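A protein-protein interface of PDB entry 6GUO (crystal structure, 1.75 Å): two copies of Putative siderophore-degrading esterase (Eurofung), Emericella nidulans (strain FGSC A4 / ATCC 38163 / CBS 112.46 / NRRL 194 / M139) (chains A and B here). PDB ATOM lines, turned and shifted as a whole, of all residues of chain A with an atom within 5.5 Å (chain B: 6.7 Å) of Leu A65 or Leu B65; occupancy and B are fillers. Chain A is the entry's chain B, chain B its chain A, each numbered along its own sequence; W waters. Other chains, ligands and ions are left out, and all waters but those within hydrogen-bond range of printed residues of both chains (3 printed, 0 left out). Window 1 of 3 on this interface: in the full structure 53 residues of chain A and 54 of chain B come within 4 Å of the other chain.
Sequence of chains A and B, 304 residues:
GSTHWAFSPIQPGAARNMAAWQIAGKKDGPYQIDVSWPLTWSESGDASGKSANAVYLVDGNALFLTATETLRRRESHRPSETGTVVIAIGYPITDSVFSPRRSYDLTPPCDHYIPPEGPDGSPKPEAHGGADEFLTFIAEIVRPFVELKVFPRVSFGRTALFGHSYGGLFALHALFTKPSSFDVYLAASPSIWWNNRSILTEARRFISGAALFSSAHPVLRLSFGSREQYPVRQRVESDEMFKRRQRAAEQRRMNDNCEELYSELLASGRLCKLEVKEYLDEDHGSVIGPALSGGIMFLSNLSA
OE1 of Glu B69 sits at hydrogen-bond distance from OG1 of Thr A66 (2.6 Å).
OE2 of Glu A69 is in hydrogen-bond range of N of Leu B65.
O of Leu A63 sits close to OE1 of Glu B69 (3.2 Å).
N of Phe B64 is in hydrogen-bond range of OE2 of Glu A69 (3.3 Å).
The backbone NH of Phe A64 sits at hydrogen-bond distance from the side-chain carboxylate of Glu B69 (3.2 Å).
OE2 of Glu B69 is in hydrogen-bond range of N of Leu A65 (2.9 Å).
OG1 of Thr B66 is in hydrogen-bond range of OE1 of Glu A69 (2.7 Å).
The backbone carbonyl oxygen (O) of Ala B62 sits close to the side-chain carboxylate (OE1) of Glu A69, at 3.1 Å.
The backbone carbonyl oxygen of Leu B63 sits close to the side-chain carboxylate of Glu A69 (3.1 Å).
OG1 of Thr A68 sits at hydrogen-bond distance from O of Phe A64, at 2.8 Å.
The backbone carbonyl oxygen of Thr B66 is in hydrogen-bond range of the side-chain hydroxyl of Thr B70 (2.7 Å).
The backbone carbonyl oxygen (O) of Thr A66 lies within hydrogen-bond range of the side-chain hydroxyl (OG1) of Thr A70, 2.7 Å away.
The backbone carbonyl oxygen (O) of Phe B64 lies within hydrogen-bond range of the side-chain hydroxyl (OG1) of Thr B68 (2.8 Å).
Among the printed residues, pairs that only touch across the chains: Ala A14 with Phe B64 (3.8 Å), Ala A14 with Leu B65 (3.8 Å), Ala A15 with Ala B15 (3.9 Å), Phe A64 with Ala B14 (3.7 Å), Leu A65 with Ala B14 (3.9 Å), Leu A65 with Leu B65 (3.8 Å) and Glu A69 with Asn B61 (3.6 Å).
Leu B65 touches three residues of chain A.
Of the printed residues of chain A, Asn B61 touches Glu A69 (3.6 Å).
Printed residues of chain B within 4 Å of Thr A66: Glu B69 (2.6 Å).
Printed residues of chain A within 4 Å of Phe B64: Ala A14 and Glu A69.
Of the printed residues of chain A, Thr B66 touches Glu A69.
Of the printed residues of chain A, Glu B69 touches Leu A63 (3.0 Å), Phe A64 (3.2 Å), Leu A65 (2.9 Å) and Thr A66 (2.6 Å).
Ala A67 touches none of the printed residues of chain B.
Ala B88 touches none of the printed residues of chain A.
The nearest residue of chain B that does not touch Leu A65 is Met B18 (4.1 Å).
The nearest residue of chain A that does not touch Leu B65 is Met A18 (4.2 Å).
The nearest printed residue of chain A that does not touch Leu B63 is Ala A14 (7.4 Å).
Hydrophobic or aromatic side chains of chain A within 4 Å of the printed part of chain B: Ala A14, Ala A15, Phe A64 and Leu A65.
Among the printed residues, no Asp or Glu carboxylate lies within 4 Å of a Lys or Arg side-chain nitrogen of the other chain.
Ala A14 touches Phe B64, and with the chains exchanged Phe A64 touches Ala B14.
Ala A14 touches Leu B65, and with the chains exchanged Leu A65 touches Ala B14.
Ala B15 touches its own counterpart, Ala A15.
Leu A63 touches Glu B69, and with the chains exchanged Glu A69 touches Leu B63.
Positions printed for both chains: 14, 15, 18, 63, 64, 65, 66, 67, 68, 69, 70 and 72.
Of the 16 pairs that touch across the chains among the printed residues, 14 have their exchanged pair printed and touching as well.
Water W1 bridges O of Asn B61 and OE2 of Glu A69.
Water W3 bridges OG1 of Thr A70 (2.7 Å) and OG1 of Thr B66 (2.8 Å).
Water W2 bridges OG1 of Thr B70 and OG1 of Thr A66.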
ATOM      1  N   ALA A  14       3.637  24.471 -27.015  1.00  0.00           N
ATOM      2  CA  ALA A  14       4.711  23.471 -26.990  1.00  0.00           C
ATOM      3  C   ALA A  14       4.474  22.341 -25.976  1.00  0.00           C
ATOM      4  O   ALA A  14       5.142  21.308 -26.044  1.00  0.00           O
ATOM      5  CB  ALA A  14       6.052  24.140 -26.722  1.00  0.00           C
ATOM      6  N   ALA A  15       3.533  22.526 -25.048  1.00  0.00           N
ATOM      7  CA  ALA A  15       3.208  21.507 -24.039  1.00  0.00           C
ATOM      8  C   ALA A  15       2.189  20.482 -24.552  1.00  0.00           C
ATOM      9  O   ALA A  15       1.222  20.161 -23.861  1.00  0.00           O
ATOM     10  CB  ALA A  15       2.694  22.178 -22.770  1.00  0.00           C
ATOM     11  N   MET A  18       1.337  15.553 -23.589  1.00  0.00           N
ATOM     12  CA  MET A  18       1.759  15.294 -22.229  1.00  0.00           C
ATOM     13  C   MET A  18       0.567  15.393 -21.286  1.00  0.00           C
ATOM     14  O   MET A  18      -0.420  16.069 -21.573  1.00  0.00           O
ATOM     15  CB  MET A  18       2.903  16.228 -21.802  1.00  0.00           C
ATOM     16  CG  MET A  18       2.611  17.710 -21.896  1.00  0.00           C
ATOM     17  SD  MET A  18       4.002  18.759 -21.413  1.00  0.00           S
ATOM     18  CE  MET A  18       5.181  18.455 -22.725  1.00  0.00           C
ATOM     19  N   LEU A  63      13.338  17.414 -14.369  1.00  0.00           N
ATOM     20  CA  LEU A  63      13.923  16.765 -15.550  1.00  0.00           C
ATOM     21  C   LEU A  63      12.949  16.459 -16.699  1.00  0.00           C
ATOM     22  O   LEU A  63      13.396  16.205 -17.817  1.00  0.00           O
ATOM     23  CB  LEU A  63      14.594  15.457 -15.119  1.00  0.00           C
ATOM     24  CG  LEU A  63      15.628  15.551 -13.991  1.00  0.00           C
ATOM     25  CD1 LEU A  63      16.101  14.155 -13.630  1.00  0.00           C
ATOM     26  CD2 LEU A  63      16.812  16.437 -14.347  1.00  0.00           C
ATOM     27  N   PHE A  64      11.640  16.508 -16.431  1.00  0.00           N
ATOM     28  CA  PHE A  64      10.601  16.056 -17.376  1.00  0.00           C
ATOM     29  C   PHE A  64      10.650  16.762 -18.732  1.00  0.00           C
ATOM     30  O   PHE A  64      10.631  16.117 -19.784  1.00  0.00           O
ATOM     31  CB  PHE A  64       9.220  16.274 -16.745  1.00  0.00           C
ATOM     32  CG  PHE A  64       8.069  15.956 -17.657  1.00  0.00           C
ATOM     33  CD1 PHE A  64       7.833  14.650 -18.072  1.00  0.00           C
ATOM     34  CD2 PHE A  64       7.214  16.958 -18.091  1.00  0.00           C
ATOM     35  CE1 PHE A  64       6.770  14.355 -18.914  1.00  0.00           C
ATOM     36  CE2 PHE A  64       6.153  16.668 -18.932  1.00  0.00           C
ATOM     37  CZ  PHE A  64       5.928  15.364 -19.337  1.00  0.00           C
ATOM     38  N   LEU A  65      10.699  18.087 -18.686  1.00  0.00           N
ATOM     39  CA  LEU A  65      10.663  18.908 -19.898  1.00  0.00           C
ATOM     40  C   LEU A  65      11.945  18.792 -20.731  1.00  0.00           C
ATOM     41  O   LEU A  65      11.880  18.766 -21.955  1.00  0.00           O
ATOM     42  CB  LEU A  65      10.379  20.371 -19.546  1.00  0.00           C
ATOM     43  CG  LEU A  65       9.077  20.656 -18.784  1.00  0.00           C
ATOM     44  CD1 LEU A  65       9.002  22.135 -18.440  1.00  0.00           C
ATOM     45  CD2 LEU A  65       7.857  20.229 -19.584  1.00  0.00           C
ATOM     46  N   THR A  66      13.092  18.698 -20.062  1.00  0.00           N
ATOM     47  CA  THR A  66      14.374  18.511 -20.735  1.00  0.00           C
ATOM     48  C   THR A  66      14.406  17.172 -21.456  1.00  0.00           C
ATOM     49  O   THR A  66      14.805  17.102 -22.619  1.00  0.00           O
ATOM     50  CB  THR A  66      15.551  18.581 -19.742  1.00  0.00           C
ATOM     51  OG1 THR A  66      15.518  19.846 -19.070  1.00  0.00           O
ATOM     52  CG2 THR A  66      16.895  18.432 -20.469  1.00  0.00           C
ATOM     53  N   ALA A  67      13.998  16.112 -20.762  1.00  0.00           N
ATOM     54  CA  ALA A  67      13.956  14.778 -21.369  1.00  0.00           C
ATOM     55  C   ALA A  67      13.015  14.762 -22.570  1.00  0.00           C
ATOM     56  O   ALA A  67      13.383  14.290 -23.647  1.00  0.00           O
ATOM     57  CB  ALA A  67      13.536  13.730 -20.353  1.00  0.00           C
ATOM     58  N   THR A  68      11.815  15.300 -22.367  1.00  0.00           N
ATOM     59  CA  THR A  68      10.788  15.392 -23.405  1.00  0.00           C
ATOM     60  C   THR A  68      11.301  16.096 -24.658  1.00  0.00           C
ATOM     61  O   THR A  68      11.174  15.574 -25.759  1.00  0.00           O
ATOM     62  CB  THR A  68       9.536  16.112 -22.856  1.00  0.00           C
ATOM     63  OG1 THR A  68       8.955  15.316 -21.814  1.00  0.00           O
ATOM     64  CG2 THR A  68       8.491  16.359 -23.938  1.00  0.00           C
ATOM     65  N   GLU A  69      11.895  17.273 -24.489  1.00  0.00           N
ATOM     66  CA  GLU A  69      12.308  18.064 -25.639  1.00  0.00           C
ATOM     67  C   GLU A  69      13.548  17.505 -26.334  1.00  0.00           C
ATOM     68  O   GLU A  69      13.647  17.584 -27.552  1.00  0.00           O
ATOM     69  CB  GLU A  69      12.515  19.526 -25.253  1.00  0.00           C
ATOM     70  CG  GLU A  69      12.440  20.442 -26.456  1.00  0.00           C
ATOM     71  CD  GLU A  69      12.345  21.889 -26.070  1.00  0.00           C
ATOM     72  OE1 GLU A  69      13.355  22.414 -25.550  1.00  0.00           O
ATOM     73  OE2 GLU A  69      11.266  22.493 -26.274  1.00  0.00           O
ATOM     74  N   THR A  70      14.479  16.927 -25.571  1.00  0.00           N
ATOM     75  CA  THR A  70      15.620  16.229 -26.164  1.00  0.00           C
ATOM     76  C   THR A  70      15.135  15.134 -27.118  1.00  0.00           C
ATOM     77  O   THR A  70      15.618  15.020 -28.249  1.00  0.00           O
ATOM     78  CB  THR A  70      16.529  15.597 -25.097  1.00  0.00           C
ATOM     79  OG1 THR A  70      16.973  16.612 -24.191  1.00  0.00           O
ATOM     80  CG2 THR A  70      17.744  14.951 -25.742  1.00  0.00           C
ATOM     81  N   ARG A  72      12.090  14.835 -28.544  1.00  0.00           N
ATOM     82  CA  ARG A  72      11.321  15.383 -29.669  1.00  0.00           C
ATOM     83  C   ARG A  72      12.199  15.982 -30.770  1.00  0.00           C
ATOM     84  O   ARG A  72      11.866  15.865 -31.951  1.00  0.00           O
ATOM     85  CB  ARG A  72      10.280  16.370 -29.165  1.00  0.00           C
ATOM     86  CG  ARG A  72       9.185  15.642 -28.421  1.00  0.00           C
ATOM     87  CD  ARG A  72       8.203  16.554 -27.736  1.00  0.00           C
ATOM     88  NE  ARG A  72       7.184  15.745 -27.081  1.00  0.00           N
ATOM     89  CZ  ARG A  72       6.080  16.215 -26.506  1.00  0.00           C
ATOM     90  NH1 ARG A  72       5.808  17.520 -26.481  1.00  0.00           N
ATOM     91  NH2 ARG A  72       5.230  15.356 -25.952  1.00  0.00           N
ATOM     92  N   ALA B  14       3.797  19.686 -14.739  1.00  0.00           N
ATOM     93  CA  ALA B  14       5.069  20.352 -15.033  1.00  0.00           C
ATOM     94  C   ALA B  14       4.950  21.500 -16.049  1.00  0.00           C
ATOM     95  O   ALA B  14       5.870  22.319 -16.160  1.00  0.00           O
ATOM     96  CB  ALA B  14       6.101  19.335 -15.503  1.00  0.00           C
ATOM     97  N   ALA B  15       3.824  21.589 -16.764  1.00  0.00           N
ATOM     98  CA  ALA B  15       3.581  22.678 -17.720  1.00  0.00           C
ATOM     99  C   ALA B  15       3.005  23.932 -17.036  1.00  0.00           C
ATOM    100  O   ALA B  15       2.070  24.563 -17.532  1.00  0.00           O
ATOM    101  CB  ALA B  15       2.663  22.199 -18.835  1.00  0.00           C
ATOM    102  N   ARG B  16       3.616  24.299 -15.915  1.00  0.00           N
ATOM    103  CA  ARG B  16       3.166  25.376 -15.050  1.00  0.00           C
ATOM    104  C   ARG B  16       3.763  26.694 -15.522  1.00  0.00           C
ATOM    105  O   ARG B  16       4.878  26.716 -16.047  1.00  0.00           O
ATOM    106  CB  ARG B  16       3.658  25.087 -13.630  1.00  0.00           C
ATOM    107  CG  ARG B  16       2.930  25.840 -12.543  1.00  0.00           C
ATOM    108  CD  ARG B  16       3.235  25.234 -11.184  1.00  0.00           C
ATOM    109  NE  ARG B  16       2.343  25.787 -10.172  1.00  0.00           N
ATOM    110  CZ  ARG B  16       1.075  25.420  -9.979  1.00  0.00           C
ATOM    111  NH1 ARG B  16       0.362  26.012  -9.024  1.00  0.00           N
ATOM    112  NH2 ARG B  16       0.505  24.468 -10.721  1.00  0.00           N
ATOM    113  N   MET B  18       3.260  28.745 -18.008  1.00  0.00           N
ATOM    114  CA  MET B  18       3.550  28.950 -19.414  1.00  0.00           C
ATOM    115  C   MET B  18       2.261  29.206 -20.176  1.00  0.00           C
ATOM    116  O   MET B  18       1.176  28.803 -19.754  1.00  0.00           O
ATOM    117  CB  MET B  18       4.357  27.790 -20.016  1.00  0.00           C
ATOM    118  CG  MET B  18       3.830  26.397 -19.748  1.00  0.00           C
ATOM    119  SD  MET B  18       4.912  25.108 -20.413  1.00  0.00           S
ATOM    120  CE  MET B  18       6.366  25.198 -19.371  1.00  0.00           C
ATOM    121  N   LEU B  57      14.284  32.865 -27.986  1.00  0.00           N
ATOM    122  CA  LEU B  57      14.749  31.670 -28.681  1.00  0.00           C
ATOM    123  C   LEU B  57      14.130  31.592 -30.072  1.00  0.00           C
ATOM    124  O   LEU B  57      12.916  31.662 -30.199  1.00  0.00           O
ATOM    125  CB  LEU B  57      14.347  30.418 -27.901  1.00  0.00           C
ATOM    126  CG  LEU B  57      14.582  30.367 -26.391  1.00  0.00           C
ATOM    127  CD1 LEU B  57      13.904  29.133 -25.811  1.00  0.00           C
ATOM    128  CD2 LEU B  57      16.062  30.350 -26.082  1.00  0.00           C
ATOM    129  N   GLY B  60      11.747  28.161 -31.897  1.00  0.00           N
ATOM    130  CA  GLY B  60      11.114  28.151 -30.580  1.00  0.00           C
ATOM    131  C   GLY B  60      10.531  26.824 -30.130  1.00  0.00           C
ATOM    132  O   GLY B  60      10.684  26.441 -28.965  1.00  0.00           O
ATOM    133  N   ASN B  61       9.892  26.112 -31.060  1.00  0.00           N
ATOM    134  CA  ASN B  61       9.234  24.838 -30.742  1.00  0.00           C
ATOM    135  C   ASN B  61      10.218  23.767 -30.265  1.00  0.00           C
ATOM    136  O   ASN B  61       9.821  22.851 -29.550  1.00  0.00           O
ATOM    137  CB  ASN B  61       8.455  24.260 -31.933  1.00  0.00           C
ATOM    138  CG  ASN B  61       7.573  25.276 -32.623  1.00  0.00           C
ATOM    139  OD1 ASN B  61       8.045  26.029 -33.464  1.00  0.00           O
ATOM    140  ND2 ASN B  61       6.284  25.280 -32.298  1.00  0.00           N
ATOM    141  N   ALA B  62      11.478  23.863 -30.694  1.00  0.00           N
ATOM    142  CA  ALA B  62      12.513  22.872 -30.365  1.00  0.00           C
ATOM    143  C   ALA B  62      13.296  23.158 -29.088  1.00  0.00           C
ATOM    144  O   ALA B  62      13.987  22.266 -28.589  1.00  0.00           O
ATOM    145  CB  ALA B  62      13.484  22.749 -31.529  1.00  0.00           C
ATOM    146  N   LEU B  63      13.213  24.389 -28.585  1.00  0.00           N
ATOM    147  CA  LEU B  63      14.076  24.874 -27.491  1.00  0.00           C
ATOM    148  C   LEU B  63      13.375  25.375 -26.230  1.00  0.00           C
ATOM    149  O   LEU B  63      14.007  25.456 -25.170  1.00  0.00           O
ATOM    150  CB  LEU B  63      14.942  26.009 -28.018  1.00  0.00           C
ATOM    151  CG  LEU B  63      15.754  25.741 -29.284  1.00  0.00           C
ATOM    152  CD1 LEU B  63      16.489  27.007 -29.675  1.00  0.00           C
ATOM    153  CD2 LEU B  63      16.726  24.594 -29.075  1.00  0.00           C
ATOM    154  N   PHE B  64      12.093  25.715 -26.343  1.00  0.00           N
ATOM    155  CA  PHE B  64      11.326  26.351 -25.271  1.00  0.00           C
ATOM    156  C   PHE B  64      11.377  25.593 -23.953  1.00  0.00           C
ATOM    157  O   PHE B  64      11.698  26.163 -22.914  1.00  0.00           O
ATOM    158  CB  PHE B  64       9.870  26.490 -25.718  1.00  0.00           C
ATOM    159  CG  PHE B  64       8.950  27.032 -24.663  1.00  0.00           C
ATOM    160  CD1 PHE B  64       9.086  28.335 -24.203  1.00  0.00           C
ATOM    161  CD2 PHE B  64       7.925  26.246 -24.151  1.00  0.00           C
ATOM    162  CE1 PHE B  64       8.222  28.845 -23.246  1.00  0.00           C
ATOM    163  CE2 PHE B  64       7.061  26.746 -23.190  1.00  0.00           C
ATOM    164  CZ  PHE B  64       7.208  28.051 -22.739  1.00  0.00           C
ATOM    165  N   LEU B  65      11.061  24.305 -24.013  1.00  0.00           N
ATOM    166  CA  LEU B  65      10.937  23.490 -22.807  1.00  0.00           C
ATOM    167  C   LEU B  65      12.284  23.287 -22.104  1.00  0.00           C
ATOM    168  O   LEU B  65      12.346  23.322 -20.874  1.00  0.00           O
ATOM    169  CB  LEU B  65      10.276  22.145 -23.130  1.00  0.00           C
ATOM    170  CG  LEU B  65       8.865  22.187 -23.734  1.00  0.00           C
ATOM    171  CD1 LEU B  65       8.408  20.783 -24.105  1.00  0.00           C
ATOM    172  CD2 LEU B  65       7.861  22.836 -22.791  1.00  0.00           C
ATOM    173  N   THR B  66      13.352  23.118 -22.882  1.00  0.00           N
ATOM    174  CA  THR B  66      14.704  22.931 -22.343  1.00  0.00           C
ATOM    175  C   THR B  66      15.167  24.203 -21.654  1.00  0.00           C
ATOM    176  O   THR B  66      15.696  24.148 -20.555  1.00  0.00           O
ATOM    177  CB  THR B  66      15.715  22.544 -23.452  1.00  0.00           C
ATOM    178  OG1 THR B  66      15.304  21.317 -24.068  1.00  0.00           O
ATOM    179  CG2 THR B  66      17.138  22.367 -22.890  1.00  0.00           C
ATOM    180  N   ALA B  67      14.970  25.349 -22.305  1.00  0.00           N
ATOM    181  CA  ALA B  67      15.335  26.633 -21.701  1.00  0.00           C
ATOM    182  C   ALA B  67      14.545  26.860 -20.409  1.00  0.00           C
ATOM    183  O   ALA B  67      15.111  27.239 -19.384  1.00  0.00           O
ATOM    184  CB  ALA B  67      15.088  27.767 -22.678  1.00  0.00           C
ATOM    185  N   THR B  68      13.241  26.597 -20.464  1.00  0.00           N
ATOM    186  CA  THR B  68      12.362  26.767 -19.309  1.00  0.00           C
ATOM    187  C   THR B  68      12.848  25.949 -18.109  1.00  0.00           C
ATOM    188  O   THR B  68      13.012  26.478 -17.004  1.00  0.00           O
ATOM    189  CB  THR B  68      10.917  26.393 -19.680  1.00  0.00           C
ATOM    190  OG1 THR B  68      10.442  27.313 -20.676  1.00  0.00           O
ATOM    191  CG2 THR B  68       9.993  26.419 -18.459  1.00  0.00           C
ATOM    192  N   GLU B  69      13.099  24.666 -18.333  1.00  0.00           N
ATOM    193  CA  GLU B  69      13.469  23.788 -17.227  1.00  0.00           C
ATOM    194  C   GLU B  69      14.871  24.058 -16.687  1.00  0.00           C
ATOM    195  O   GLU B  69      15.080  23.987 -15.477  1.00  0.00           O
ATOM    196  CB  GLU B  69      13.330  22.334 -17.619  1.00  0.00           C
ATOM    197  CG  GLU B  69      13.238  21.423 -16.412  1.00  0.00           C
ATOM    198  CD  GLU B  69      12.716  20.070 -16.791  1.00  0.00           C
ATOM    199  OE1 GLU B  69      13.469  19.351 -17.470  1.00  0.00           O
ATOM    200  OE2 GLU B  69      11.561  19.740 -16.440  1.00  0.00           O
ATOM    201  N   THR B  70      15.822  24.364 -17.569  1.00  0.00           N
ATOM    202  CA  THR B  70      17.164  24.739 -17.134  1.00  0.00           C
ATOM    203  C   THR B  70      17.113  25.928 -16.178  1.00  0.00           C
ATOM    204  O   THR B  70      17.763  25.917 -15.130  1.00  0.00           O
ATOM    205  CB  THR B  70      18.083  25.082 -18.324  1.00  0.00           C
ATOM    206  OG1 THR B  70      18.064  24.014 -19.279  1.00  0.00           O
ATOM    207  CG2 THR B  70      19.501  25.305 -17.847  1.00  0.00           C
ATOM    208  N   ARG B  72      14.460  26.910 -14.394  1.00  0.00           N
ATOM    209  CA  ARG B  72      13.720  26.553 -13.183  1.00  0.00           C
ATOM    210  C   ARG B  72      14.562  25.742 -12.196  1.00  0.00           C
ATOM    211  O   ARG B  72      14.425  25.927 -10.992  1.00  0.00           O
ATOM    212  CB  ARG B  72      12.411  25.849 -13.524  1.00  0.00           C
ATOM    213  CG  ARG B  72      11.407  26.839 -14.084  1.00  0.00           C
ATOM    214  CD  ARG B  72      10.175  26.193 -14.676  1.00  0.00           C
ATOM    215  NE  ARG B  72       9.303  27.238 -15.204  1.00  0.00           N
ATOM    216  CZ  ARG B  72       8.064  27.063 -15.661  1.00  0.00           C
ATOM    217  NH1 ARG B  72       7.497  25.859 -15.675  1.00  0.00           N
ATOM    218  NH2 ARG B  72       7.380  28.120 -16.106  1.00  0.00           N
ATOM    219  N   VAL B  86      11.204  33.239 -20.556  1.00  0.00           N
ATOM    220  CA  VAL B  86      11.585  32.612 -21.822  1.00  0.00           C
ATOM    221  C   VAL B  86      10.529  32.973 -22.851  1.00  0.00           C
ATOM    222  O   VAL B  86       9.334  32.825 -22.591  1.00  0.00           O
ATOM    223  CB  VAL B  86      11.672  31.077 -21.708  1.00  0.00           C
ATOM    224  CG1 VAL B  86      12.053  30.445 -23.043  1.00  0.00           C
ATOM    225  CG2 VAL B  86      12.670  30.680 -20.633  1.00  0.00           C
ATOM    226  N   ALA B  88       9.894  31.971 -26.738  1.00  0.00           N
ATOM    227  CA  ALA B  88      10.266  31.112 -27.846  1.00  0.00           C
ATOM    228  C   ALA B  88       9.444  31.515 -29.055  1.00  0.00           C
ATOM    229  O   ALA B  88       8.224  31.521 -28.984  1.00  0.00           O
ATOM    230  CB  ALA B  88      10.005  29.663 -27.485  1.00  0.00           C
ATOM    231  N   LEU B 292      22.456  24.902 -25.218  1.00  0.00           N
ATOM    232  CA  LEU B 292      21.377  25.734 -24.679  1.00  0.00           C
ATOM    233  C   LEU B 292      21.502  25.851 -23.165  1.00  0.00           C
ATOM    234  O   LEU B 292      21.479  26.959 -22.628  1.00  0.00           O
ATOM    235  CB  LEU B 292      20.006  25.193 -25.074  1.00  0.00           C
ATOM    236  CG  LEU B 292      18.773  25.945 -24.558  1.00  0.00           C
ATOM    237  CD1 LEU B 292      18.834  27.452 -24.802  1.00  0.00           C
ATOM    238  CD2 LEU B 292      17.548  25.357 -25.223  1.00  0.00           C
HETATM  239  O   HOH W   1       9.297  21.167 -27.586  1.00  0.00           O
HETATM  240  O   HOH W   2      18.277  21.353 -19.455  1.00  0.00           O
HETATM  241  O   HOH W   3      17.250  19.259 -23.955  1.00  0.00           O
